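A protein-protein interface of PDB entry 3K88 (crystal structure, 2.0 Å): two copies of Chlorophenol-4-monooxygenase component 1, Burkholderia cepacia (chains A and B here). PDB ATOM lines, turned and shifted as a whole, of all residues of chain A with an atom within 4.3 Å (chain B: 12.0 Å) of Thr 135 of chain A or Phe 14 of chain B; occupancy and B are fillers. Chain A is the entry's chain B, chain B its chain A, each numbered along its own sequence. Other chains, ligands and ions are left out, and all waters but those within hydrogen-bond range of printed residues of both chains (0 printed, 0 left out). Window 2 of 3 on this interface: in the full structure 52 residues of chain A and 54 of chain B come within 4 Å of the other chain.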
ATOM      1  N   GLY A  80      12.924   2.529  -6.599  1.00  0.00           N
ATOM      2  CA  GLY A  80      12.201   1.444  -7.309  1.00  0.00           C
ATOM      3  C   GLY A  80      13.090   0.730  -8.333  1.00  0.00           C
ATOM      4  O   GLY A  80      12.655  -0.203  -9.019  1.00  0.00           O
ATOM      5  N   ALA A 119      19.396   1.388 -18.720  1.00  0.00           N
ATOM      6  CA  ALA A 119      17.945   1.466 -18.993  1.00  0.00           C
ATOM      7  C   ALA A 119      17.120   2.184 -17.924  1.00  0.00           C
ATOM      8  O   ALA A 119      16.266   3.015 -18.223  1.00  0.00           O
ATOM      9  CB  ALA A 119      17.388   0.094 -19.251  1.00  0.00           C
ATOM     10  N   THR A 120      17.369   1.888 -16.673  1.00  0.00           N
ATOM     11  CA  THR A 120      16.484   2.363 -15.617  1.00  0.00           C
ATOM     12  C   THR A 120      16.834   3.742 -15.065  1.00  0.00           C
ATOM     13  O   THR A 120      16.010   4.354 -14.424  1.00  0.00           O
ATOM     14  CB  THR A 120      16.511   1.387 -14.420  1.00  0.00           C
ATOM     15  OG1 THR A 120      17.792   1.468 -13.765  1.00  0.00           O
ATOM     16  CG2 THR A 120      16.190  -0.083 -14.884  1.00  0.00           C
ATOM     17  N   CYS A 134      18.128  -3.175 -13.091  1.00  0.00           N
ATOM     18  CA  CYS A 134      16.936  -3.907 -12.586  1.00  0.00           C
ATOM     19  C   CYS A 134      15.817  -3.023 -12.136  1.00  0.00           C
ATOM     20  O   CYS A 134      16.031  -1.882 -11.776  1.00  0.00           O
ATOM     21  CB  CYS A 134      17.283  -4.862 -11.423  1.00  0.00           C
ATOM     22  SG  CYS A 134      18.793  -5.879 -11.654  1.00  0.00           S
ATOM     23  N   THR A 135      14.611  -3.575 -12.099  1.00  0.00           N
ATOM     24  CA  THR A 135      13.522  -2.912 -11.393  1.00  0.00           C
ATOM     25  C   THR A 135      13.085  -3.787 -10.262  1.00  0.00           C
ATOM     26  O   THR A 135      12.934  -4.990 -10.438  1.00  0.00           O
ATOM     27  CB  THR A 135      12.196  -2.760 -12.327  1.00  0.00           C
ATOM     28  OG1 THR A 135      11.897  -4.032 -12.950  1.00  0.00           O
ATOM     29  CG2 THR A 135      12.436  -1.808 -13.443  1.00  0.00           C
ATOM     30  N   ILE A 136      12.763  -3.175  -9.136  1.00  0.00           N
ATOM     31  CA  ILE A 136      12.281  -3.901  -7.993  1.00  0.00           C
ATOM     32  C   ILE A 136      10.907  -4.527  -8.302  1.00  0.00           C
ATOM     33  O   ILE A 136      10.024  -3.826  -8.803  1.00  0.00           O
ATOM     34  CB  ILE A 136      12.249  -2.942  -6.735  1.00  0.00           C
ATOM     35  CG1 ILE A 136      13.660  -2.464  -6.483  1.00  0.00           C
ATOM     36  CG2 ILE A 136      11.593  -3.613  -5.512  1.00  0.00           C
ATOM     37  CD1 ILE A 136      13.835  -1.577  -5.179  1.00  0.00           C
ATOM     38  N   ALA A 137      10.714  -5.812  -7.945  1.00  0.00           N
ATOM     39  CA  ALA A 137       9.404  -6.496  -8.108  1.00  0.00           C
ATOM     40  C   ALA A 137       8.725  -6.852  -6.762  1.00  0.00           C
ATOM     41  O   ALA A 137       7.524  -6.945  -6.656  1.00  0.00           O
ATOM     42  CB  ALA A 137       9.629  -7.771  -8.908  1.00  0.00           C
ATOM     43  N   ALA A 150      14.584  -8.229  -7.573  1.00  0.00           N
ATOM     44  CA  ALA A 150      14.616  -7.293  -8.705  1.00  0.00           C
ATOM     45  C   ALA A 150      14.649  -8.029 -10.043  1.00  0.00           C
ATOM     46  O   ALA A 150      15.450  -8.970 -10.205  1.00  0.00           O
ATOM     47  CB  ALA A 150      15.850  -6.405  -8.593  1.00  0.00           C
ATOM     48  N   GLU A 151      13.824  -7.604 -11.003  1.00  0.00           N
ATOM     49  CA  GLU A 151      13.916  -8.167 -12.339  1.00  0.00           C
ATOM     50  C   GLU A 151      14.907  -7.448 -13.245  1.00  0.00           C
ATOM     51  O   GLU A 151      14.939  -6.208 -13.321  1.00  0.00           O
ATOM     52  CB  GLU A 151      12.534  -8.191 -12.960  1.00  0.00           C
ATOM     53  CG  GLU A 151      11.680  -9.136 -12.137  1.00  0.00           C
ATOM     54  CD  GLU A 151      10.228  -9.144 -12.575  1.00  0.00           C
ATOM     55  OE1 GLU A 151       9.895  -8.338 -13.482  1.00  0.00           O
ATOM     56  OE2 GLU A 151       9.418  -9.937 -12.012  1.00  0.00           O
ATOM     57  N   VAL A 153      16.500  -5.920 -16.455  1.00  0.00           N
ATOM     58  CA  VAL A 153      16.030  -5.357 -17.709  1.00  0.00           C
ATOM     59  C   VAL A 153      17.165  -5.050 -18.664  1.00  0.00           C
ATOM     60  O   VAL A 153      16.910  -4.909 -19.832  1.00  0.00           O
ATOM     61  CB  VAL A 153      15.129  -4.111 -17.531  1.00  0.00           C
ATOM     62  CG1 VAL A 153      14.003  -4.404 -16.510  1.00  0.00           C
ATOM     63  CG2 VAL A 153      15.940  -2.907 -17.115  1.00  0.00           C
ATOM     64  N   PHE B  14       9.806  -1.307 -19.253  1.00  0.00           N
ATOM     65  CA  PHE B  14      11.067  -2.006 -19.538  1.00  0.00           C
ATOM     66  C   PHE B  14      10.791  -3.451 -19.835  1.00  0.00           C
ATOM     67  O   PHE B  14       9.937  -4.060 -19.203  1.00  0.00           O
ATOM     68  CB  PHE B  14      12.027  -1.927 -18.354  1.00  0.00           C
ATOM     69  CG  PHE B  14      12.419  -0.530 -17.995  1.00  0.00           C
ATOM     70  CD1 PHE B  14      13.325   0.169 -18.778  1.00  0.00           C
ATOM     71  CD2 PHE B  14      11.875   0.094 -16.885  1.00  0.00           C
ATOM     72  CE1 PHE B  14      13.681   1.461 -18.464  1.00  0.00           C
ATOM     73  CE2 PHE B  14      12.242   1.412 -16.564  1.00  0.00           C
ATOM     74  CZ  PHE B  14      13.133   2.087 -17.368  1.00  0.00           C
ATOM     75  N   GLU B  15      11.503  -4.000 -20.811  1.00  0.00           N
ATOM     76  CA  GLU B  15      11.424  -5.436 -21.070  1.00  0.00           C
ATOM     77  C   GLU B  15      12.587  -6.148 -20.412  1.00  0.00           C
ATOM     78  O   GLU B  15      13.747  -5.694 -20.437  1.00  0.00           O
ATOM     79  CB  GLU B  15      11.452  -5.762 -22.561  1.00  0.00           C
ATOM     80  CG  GLU B  15      10.186  -5.450 -23.344  1.00  0.00           C
ATOM     81  CD  GLU B  15      10.324  -5.875 -24.807  1.00  0.00           C
ATOM     82  OE1 GLU B  15      10.829  -7.003 -25.052  1.00  0.00           O
ATOM     83  OE2 GLU B  15       9.945  -5.076 -25.702  1.00  0.00           O
ATOM     84  N   THR B  16      12.263  -7.306 -19.871  1.00  0.00           N
ATOM     85  CA  THR B  16      13.219  -8.115 -19.149  1.00  0.00           C
ATOM     86  C   THR B  16      14.169  -8.807 -20.168  1.00  0.00           C
ATOM     87  O   THR B  16      13.780  -9.023 -21.316  1.00  0.00           O
ATOM     88  CB  THR B  16      12.388  -9.024 -18.190  1.00  0.00           C
ATOM     89  OG1 THR B  16      13.090  -9.224 -16.961  1.00  0.00           O
ATOM     90  CG2 THR B  16      11.972 -10.299 -18.824  1.00  0.00           C
ATOM     91  N   VAL B  17      15.439  -9.049 -19.814  1.00  0.00           N
ATOM     92  CA  VAL B  17      16.392  -9.670 -20.748  1.00  0.00           C
ATOM     93  C   VAL B  17      15.959 -11.115 -21.115  1.00  0.00           C
ATOM     94  O   VAL B  17      15.167 -11.710 -20.415  1.00  0.00           O
ATOM     95  CB  VAL B  17      17.846  -9.667 -20.187  1.00  0.00           C
ATOM     96  CG1 VAL B  17      18.372  -8.234 -19.970  1.00  0.00           C
ATOM     97  CG2 VAL B  17      17.961 -10.503 -18.897  1.00  0.00           C
ATOM     98  N   ALA B  18      16.460 -11.656 -22.219  1.00  0.00           N
ATOM     99  CA  ALA B  18      16.245 -13.053 -22.572  1.00  0.00           C
ATOM    100  C   ALA B  18      16.852 -13.941 -21.504  1.00  0.00           C
ATOM    101  O   ALA B  18      17.946 -13.671 -21.019  1.00  0.00           O
ATOM    102  CB  ALA B  18      16.950 -13.380 -23.950  1.00  0.00           C
ATOM    103  N   PHE B  22      20.609 -13.853 -19.658  1.00  0.00           N
ATOM    104  CA  PHE B  22      20.735 -13.761 -18.197  1.00  0.00           C
ATOM    105  C   PHE B  22      21.688 -14.858 -17.621  1.00  0.00           C
ATOM    106  O   PHE B  22      22.609 -14.583 -16.849  1.00  0.00           O
ATOM    107  CB  PHE B  22      19.318 -13.892 -17.604  1.00  0.00           C
ATOM    108  CG  PHE B  22      19.274 -14.022 -16.102  1.00  0.00           C
ATOM    109  CD1 PHE B  22      19.401 -12.882 -15.277  1.00  0.00           C
ATOM    110  CD2 PHE B  22      19.028 -15.261 -15.505  1.00  0.00           C
ATOM    111  CE1 PHE B  22      19.307 -12.979 -13.887  1.00  0.00           C
ATOM    112  CE2 PHE B  22      18.912 -15.374 -14.130  1.00  0.00           C
ATOM    113  CZ  PHE B  22      19.055 -14.270 -13.309  1.00  0.00           C
ATOM    114  N   VAL B 142       9.118 -17.911  -6.569  1.00  0.00           N
ATOM    115  CA  VAL B 142       9.428 -16.986  -7.628  1.00  0.00           C
ATOM    116  C   VAL B 142       9.758 -17.752  -8.927  1.00  0.00           C
ATOM    117  O   VAL B 142      10.730 -18.487  -9.004  1.00  0.00           O
ATOM    118  CB  VAL B 142      10.652 -16.116  -7.225  1.00  0.00           C
ATOM    119  CG1 VAL B 142      10.795 -14.933  -8.176  1.00  0.00           C
ATOM    120  CG2 VAL B 142      10.529 -15.666  -5.712  1.00  0.00           C
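The backbone carbonyl oxygen (O) of Val 153 of chain A sits close to the backbone carbonyl oxygen (O) of Glu 15 of chain B (3.3 Å).
The backbone carbonyl oxygen (O) of Thr 135 of chain A sits at hydrogen-bond distance from the backbone NH (N) of Glu 151 of chain A (2.8 Å).
Phe 14 of chain B touches Ala 119 of chain A.
CA of Thr 120 of chain A touches CZ of Phe 14 of chain B, at 3.8 Å.
Thr 135 of chain A touches Phe 14 of chain B (CG2 to CD2, 3.97 Å).
Val 153 of chain A touches Phe 14 of chain B (CG1 to CB, 3.7 Å).
O of Val 153 of chain A touches CG1 of Val 17 of chain B (3.6 Å).
Gly 80 of chain A touches none of the printed residues of chain B.
Of chain B, only Phe 14 (3.0 Å) comes within 4 Å of Ala 119 of chain A.
Of chain B, only Phe 14 comes within 4 Å of Thr 120 of chain A.
No residue of chain B comes within 4 Å of Cys 134 of chain A.
Thr 135 of chain A touches just one residue of chain B: Phe 14.
Ile 136 of chain A touches none of the printed residues of chain B.
No residue of chain B comes within 4 Å of Ala 137 of chain A.
No residue of chain B comes within 4 Å of Ala 150 of chain A.
No residue of chain B comes within 4 Å of Glu 151 of chain A.
Val 153 of chain A touches three residues of chain B.
Printed residues of chain A within 4 Å of Phe 14 of chain B: Ala 119 (3.0 Å), Thr 120 (3.8 Å), Thr 135 (3.97 Å) and Val 153 (3.7 Å).
Of the printed residues of chain A, Glu 15 of chain B touches Val 153.
Thr 16 of chain B touches none of the printed residues of chain A.
Of the printed residues of chain A, Val 17 of chain B touches Val 153.
The nearest residue of chain B that does not touch Thr 135 of chain A is Thr 16 of chain B (6.7 Å).
The nearest printed residue of chain A that does not touch Val 17 of chain B is Glu 151 of chain A (6.8 Å).
Of the 10 printed residues of chain A, 4 touch a printed residue of chain B.
Printed residues of chain A that touch a printed residue of chain B: Ala 119, Thr 120, Thr 135 and Val 153.
Hydrophobic or aromatic side chains of chain A that line the printed part of chain B: Val 153.
Along chain A the printed residues that touch a printed residue of chain B span positions 119 to 153.
Of the 7 printed residues of chain B, 3 touch a printed residue of chain A.
Hydrophobic or aromatic side chains of chain B that line the printed part of chain A: Phe 14 and Val 17.
Among the printed residues, no Asp or Glu carboxylate lies within 4 Å of a Lys or Arg side-chain nitrogen of the other chain.
No position is printed for both chains.
Of the 6 pairs that touch across the chains among the printed residues, none has its exchanged pair printed and touching as well.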
